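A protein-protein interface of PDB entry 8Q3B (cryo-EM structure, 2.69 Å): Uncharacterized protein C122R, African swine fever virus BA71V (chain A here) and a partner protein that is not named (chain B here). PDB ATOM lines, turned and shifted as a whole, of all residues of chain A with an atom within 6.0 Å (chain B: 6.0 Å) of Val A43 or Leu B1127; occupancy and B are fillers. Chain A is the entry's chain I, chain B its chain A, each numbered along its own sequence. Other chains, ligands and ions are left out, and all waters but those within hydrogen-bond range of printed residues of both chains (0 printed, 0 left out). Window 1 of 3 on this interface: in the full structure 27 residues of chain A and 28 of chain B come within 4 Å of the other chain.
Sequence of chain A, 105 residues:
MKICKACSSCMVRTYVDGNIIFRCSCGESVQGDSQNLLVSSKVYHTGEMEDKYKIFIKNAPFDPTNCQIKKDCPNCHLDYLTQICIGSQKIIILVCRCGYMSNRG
The backbone carbonyl oxygen (O) of Leu B1127 lies within hydrogen-bond range of the backbone NH (N) of Tyr A44 (2.7 Å).
N of Trp B1129 is in hydrogen-bond range of O of Lys A42, 3.0 Å away.
A ring nitrogen (ND1) of His B1130 sits at hydrogen-bond distance from the side-chain hydroxyl (OG) of Ser A41 (3.2 Å).
O of Glu B1179 lies within hydrogen-bond range of N of Leu B1127 (2.6 Å).
NE2 of His B1130 lies within hydrogen-bond range of NE2 of Gln B1128, at 3.3 Å.
The backbone carbonyl oxygen (O) of Gln B1128 is in hydrogen-bond range of the backbone NH (N) of Glu B1179 (2.9 Å).
OG1 of Thr A46 sits at hydrogen-bond distance from O of Val A43, at 3.2 Å.
Among the printed residues, pairs that only touch across the chains: Ser A41 with Trp B1129, Lys A42 with Gln B1128, Val A43 with Leu B1127, Val A43 with Gln B1128, Tyr A44 with Ile B1126 and Tyr A44 with Trp B1129.
Printed residues of chain B within 4 Å of Ser A41: Trp B1129 (3.3 Å) and His B1130 (3.2 Å).
Of chain B, only Leu B1127 (3.6 Å) and Gln B1128 (3.8 Å) come within 4 Å of Val A43.
Printed residues of chain A within 4 Å of His B1130: Ser A41 (3.2 Å).
Glu B1179 touches none of the printed residues of chain A.
Leu B1180 touches none of the printed residues of chain A.
The nearest residue of chain B that does not touch Val A43 is His B1130 (5.0 Å).
Of the 10 printed residues of chain B, 5 touch a printed residue of chain A.
Hydrophobic or aromatic side chains of chain B that line the printed part of chain A: Ile B1126, Trp B1129 and His B1130.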
ATOM      1  N   SER A  41      11.416 -17.162  12.223  1.00  0.00           N
ATOM      2  CA  SER A  41      11.273 -17.916  10.984  1.00  0.00           C
ATOM      3  C   SER A  41      12.456 -18.862  10.845  1.00  0.00           C
ATOM      4  O   SER A  41      13.422 -18.801  11.609  1.00  0.00           O
ATOM      5  CB  SER A  41      11.177 -16.985   9.775  1.00  0.00           C
ATOM      6  OG  SER A  41      11.712 -17.600   8.617  1.00  0.00           O
ATOM      7  N   LYS A  42      12.359 -19.743   9.853  1.00  0.00           N
ATOM      8  CA  LYS A  42      13.424 -20.686   9.545  1.00  0.00           C
ATOM      9  C   LYS A  42      13.162 -21.308   8.181  1.00  0.00           C
ATOM     10  O   LYS A  42      12.069 -21.821   7.926  1.00  0.00           O
ATOM     11  CB  LYS A  42      13.518 -21.752  10.644  1.00  0.00           C
ATOM     12  CG  LYS A  42      14.130 -23.094  10.235  1.00  0.00           C
ATOM     13  CD  LYS A  42      15.646 -23.029  10.162  1.00  0.00           C
ATOM     14  CE  LYS A  42      16.273 -24.342  10.603  1.00  0.00           C
ATOM     15  NZ  LYS A  42      16.265 -24.494  12.084  1.00  0.00           N
ATOM     16  N   VAL A  43      14.157 -21.267   7.300  1.00  0.00           N
ATOM     17  CA  VAL A  43      14.060 -21.843   5.964  1.00  0.00           C
ATOM     18  C   VAL A  43      14.982 -23.052   5.937  1.00  0.00           C
ATOM     19  O   VAL A  43      16.195 -22.926   6.151  1.00  0.00           O
ATOM     20  CB  VAL A  43      14.427 -20.827   4.875  1.00  0.00           C
ATOM     21  CG1 VAL A  43      14.328 -21.465   3.498  1.00  0.00           C
ATOM     22  CG2 VAL A  43      13.528 -19.603   4.968  1.00  0.00           C
ATOM     23  N   TYR A  44      14.409 -24.227   5.676  1.00  0.00           N
ATOM     24  CA  TYR A  44      15.153 -25.465   5.874  1.00  0.00           C
ATOM     25  C   TYR A  44      16.160 -25.703   4.757  1.00  0.00           C
ATOM     26  O   TYR A  44      17.246 -26.243   4.998  1.00  0.00           O
ATOM     27  CB  TYR A  44      14.179 -26.637   5.993  1.00  0.00           C
ATOM     28  CG  TYR A  44      13.677 -26.820   7.403  1.00  0.00           C
ATOM     29  CD1 TYR A  44      14.536 -27.213   8.419  1.00  0.00           C
ATOM     30  CD2 TYR A  44      12.351 -26.571   7.727  1.00  0.00           C
ATOM     31  CE1 TYR A  44      14.088 -27.371   9.710  1.00  0.00           C
ATOM     32  CE2 TYR A  44      11.894 -26.726   9.017  1.00  0.00           C
ATOM     33  CZ  TYR A  44      12.768 -27.124  10.003  1.00  0.00           C
ATOM     34  OH  TYR A  44      12.322 -27.280  11.292  1.00  0.00           O
ATOM     35  N   HIS A  45      15.827 -25.307   3.528  1.00  0.00           N
ATOM     36  CA  HIS A  45      16.741 -25.489   2.399  1.00  0.00           C
ATOM     37  C   HIS A  45      17.754 -24.341   2.418  1.00  0.00           C
ATOM     38  O   HIS A  45      17.728 -23.408   1.614  1.00  0.00           O
ATOM     39  CB  HIS A  45      15.963 -25.577   1.089  1.00  0.00           C
ATOM     40  CG  HIS A  45      16.766 -25.239  -0.132  1.00  0.00           C
ATOM     41  ND1 HIS A  45      17.254 -23.973  -0.380  1.00  0.00           N
ATOM     42  CD2 HIS A  45      17.179 -26.009  -1.165  1.00  0.00           C
ATOM     43  CE1 HIS A  45      17.923 -23.977  -1.518  1.00  0.00           C
ATOM     44  NE2 HIS A  45      17.894 -25.201  -2.014  1.00  0.00           N
ATOM     45  N   THR A  46      18.647 -24.406   3.407  1.00  0.00           N
ATOM     46  CA  THR A  46      19.745 -23.448   3.468  1.00  0.00           C
ATOM     47  C   THR A  46      20.809 -23.774   2.429  1.00  0.00           C
ATOM     48  O   THR A  46      21.357 -22.870   1.787  1.00  0.00           O
ATOM     49  CB  THR A  46      20.354 -23.434   4.870  1.00  0.00           C
ATOM     50  OG1 THR A  46      19.321 -23.230   5.842  1.00  0.00           O
ATOM     51  CG2 THR A  46      21.390 -22.324   4.996  1.00  0.00           C
ATOM     52  N   LEU B1125       8.667 -32.406   6.034  1.00  0.00           N
ATOM     53  CA  LEU B1125       7.708 -32.219   4.954  1.00  0.00           C
ATOM     54  C   LEU B1125       7.489 -30.751   4.612  1.00  0.00           C
ATOM     55  O   LEU B1125       6.540 -30.429   3.891  1.00  0.00           O
ATOM     56  CB  LEU B1125       6.371 -32.867   5.319  1.00  0.00           C
ATOM     57  CG  LEU B1125       6.358 -34.391   5.454  1.00  0.00           C
ATOM     58  CD1 LEU B1125       4.969 -34.869   5.836  1.00  0.00           C
ATOM     59  CD2 LEU B1125       6.819 -35.065   4.171  1.00  0.00           C
ATOM     60  N   ILE B1126       8.343 -29.855   5.108  1.00  0.00           N
ATOM     61  CA  ILE B1126       8.170 -28.422   4.921  1.00  0.00           C
ATOM     62  C   ILE B1126       9.483 -27.815   4.445  1.00  0.00           C
ATOM     63  O   ILE B1126      10.568 -28.349   4.685  1.00  0.00           O
ATOM     64  CB  ILE B1126       7.699 -27.725   6.215  1.00  0.00           C
ATOM     65  CG1 ILE B1126       8.723 -27.933   7.333  1.00  0.00           C
ATOM     66  CG2 ILE B1126       6.338 -28.258   6.629  1.00  0.00           C
ATOM     67  CD1 ILE B1126       8.249 -27.486   8.698  1.00  0.00           C
ATOM     68  N   LEU B1127       9.366 -26.679   3.759  1.00  0.00           N
ATOM     69  CA  LEU B1127      10.516 -25.900   3.320  1.00  0.00           C
ATOM     70  C   LEU B1127      10.843 -24.752   4.263  1.00  0.00           C
ATOM     71  O   LEU B1127      12.020 -24.467   4.499  1.00  0.00           O
ATOM     72  CB  LEU B1127      10.277 -25.340   1.914  1.00  0.00           C
ATOM     73  CG  LEU B1127      10.058 -26.368   0.806  1.00  0.00           C
ATOM     74  CD1 LEU B1127       8.894 -25.969  -0.086  1.00  0.00           C
ATOM     75  CD2 LEU B1127      11.325 -26.543  -0.015  1.00  0.00           C
ATOM     76  N   GLN B1128       9.827 -24.083   4.804  1.00  0.00           N
ATOM     77  CA  GLN B1128      10.051 -22.978   5.723  1.00  0.00           C
ATOM     78  C   GLN B1128       8.826 -22.813   6.608  1.00  0.00           C
ATOM     79  O   GLN B1128       7.708 -23.186   6.234  1.00  0.00           O
ATOM     80  CB  GLN B1128      10.352 -21.677   4.972  1.00  0.00           C
ATOM     81  CG  GLN B1128       9.136 -21.052   4.310  1.00  0.00           C
ATOM     82  CD  GLN B1128       9.458 -20.407   2.977  1.00  0.00           C
ATOM     83  OE1 GLN B1128      10.205 -20.961   2.170  1.00  0.00           O
ATOM     84  NE2 GLN B1128       8.895 -19.229   2.738  1.00  0.00           N
ATOM     85  N   TRP B1129       9.056 -22.250   7.795  1.00  0.00           N
ATOM     86  CA  TRP B1129       7.988 -21.951   8.736  1.00  0.00           C
ATOM     87  C   TRP B1129       8.221 -20.576   9.339  1.00  0.00           C
ATOM     88  O   TRP B1129       9.349 -20.230   9.701  1.00  0.00           O
ATOM     89  CB  TRP B1129       7.896 -23.007   9.847  1.00  0.00           C
ATOM     90  CG  TRP B1129       9.071 -23.071  10.767  1.00  0.00           C
ATOM     91  CD1 TRP B1129      10.143 -23.907  10.669  1.00  0.00           C
ATOM     92  CD2 TRP B1129       9.283 -22.282  11.944  1.00  0.00           C
ATOM     93  NE1 TRP B1129      11.013 -23.684  11.707  1.00  0.00           N
ATOM     94  CE2 TRP B1129      10.509 -22.690  12.503  1.00  0.00           C
ATOM     95  CE3 TRP B1129       8.559 -21.268  12.574  1.00  0.00           C
ATOM     96  CZ2 TRP B1129      11.026 -22.118  13.661  1.00  0.00           C
ATOM     97  CZ3 TRP B1129       9.074 -20.702  13.724  1.00  0.00           C
ATOM     98  CH2 TRP B1129      10.296 -21.128  14.256  1.00  0.00           C
ATOM     99  N   HIS B1130       7.147 -19.798   9.442  1.00  0.00           N
ATOM    100  CA  HIS B1130       7.194 -18.438   9.966  1.00  0.00           C
ATOM    101  C   HIS B1130       6.183 -18.299  11.093  1.00  0.00           C
ATOM    102  O   HIS B1130       5.009 -18.635  10.920  1.00  0.00           O
ATOM    103  CB  HIS B1130       6.888 -17.410   8.872  1.00  0.00           C
ATOM    104  CG  HIS B1130       7.791 -17.500   7.683  1.00  0.00           C
ATOM    105  ND1 HIS B1130       8.867 -16.659   7.500  1.00  0.00           N
ATOM    106  CD2 HIS B1130       7.775 -18.329   6.613  1.00  0.00           C
ATOM    107  CE1 HIS B1130       9.477 -16.967   6.370  1.00  0.00           C
ATOM    108  NE2 HIS B1130       8.835 -17.977   5.811  1.00  0.00           N
ATOM    109  N   GLU B1179       5.349 -23.825   4.585  1.00  0.00           N
ATOM    110  CA  GLU B1179       5.412 -24.097   3.153  1.00  0.00           C
ATOM    111  C   GLU B1179       5.828 -25.550   2.970  1.00  0.00           C
ATOM    112  O   GLU B1179       6.902 -25.954   3.426  1.00  0.00           O
ATOM    113  CB  GLU B1179       6.392 -23.148   2.464  1.00  0.00           C
ATOM    114  CG  GLU B1179       6.838 -23.572   1.070  1.00  0.00           C
ATOM    115  CD  GLU B1179       6.648 -22.478   0.037  1.00  0.00           C
ATOM    116  OE1 GLU B1179       6.388 -22.811  -1.137  1.00  0.00           O
ATOM    117  OE2 GLU B1179       6.763 -21.288   0.395  1.00  0.00           O
ATOM    118  N   LEU B1180       4.980 -26.328   2.303  1.00  0.00           N
ATOM    119  CA  LEU B1180       5.199 -27.759   2.150  1.00  0.00           C
ATOM    120  C   LEU B1180       6.054 -28.046   0.921  1.00  0.00           C
ATOM    121  O   LEU B1180       5.980 -27.344  -0.091  1.00  0.00           O
ATOM    122  CB  LEU B1180       3.862 -28.496   2.039  1.00  0.00           C
ATOM    123  CG  LEU B1180       3.356 -29.165   3.320  1.00  0.00           C
ATOM    124  CD1 LEU B1180       3.207 -28.156   4.447  1.00  0.00           C
ATOM    125  CD2 LEU B1180       2.036 -29.871   3.068  1.00  0.00           C
ATOM    126  N   ASN B1181       6.872 -29.092   1.022  1.00  0.00           N
ATOM    127  CA  ASN B1181       7.762 -29.498  -0.060  1.00  0.00           C
ATOM    128  C   ASN B1181       7.066 -30.578  -0.880  1.00  0.00           C
ATOM    129  O   ASN B1181       6.905 -31.710  -0.417  1.00  0.00           O
ATOM    130  CB  ASN B1181       9.089 -30.005   0.500  1.00  0.00           C
ATOM    131  CG  ASN B1181      10.095 -30.329  -0.586  1.00  0.00           C
ATOM    132  OD1 ASN B1181       9.795 -30.229  -1.775  1.00  0.00           O
ATOM    133  ND2 ASN B1181      11.299 -30.712  -0.180  1.00  0.00           N
ATOM    134  N   LYS B1182       6.671 -30.235  -2.108  1.00  0.00           N
ATOM    135  CA  LYS B1182       5.939 -31.188  -2.938  1.00  0.00           C
ATOM    136  C   LYS B1182       6.807 -32.381  -3.316  1.00  0.00           C
ATOM    137  O   LYS B1182       6.314 -33.512  -3.391  1.00  0.00           O
ATOM    138  CB  LYS B1182       5.411 -30.500  -4.195  1.00  0.00           C
ATOM    139  CG  LYS B1182       4.445 -29.363  -3.922  1.00  0.00           C
ATOM    140  CD  LYS B1182       3.948 -28.749  -5.217  1.00  0.00           C
ATOM    141  CE  LYS B1182       3.029 -27.574  -4.955  1.00  0.00           C
ATOM    142  NZ  LYS B1182       2.591 -26.917  -6.216  1.00  0.00           N
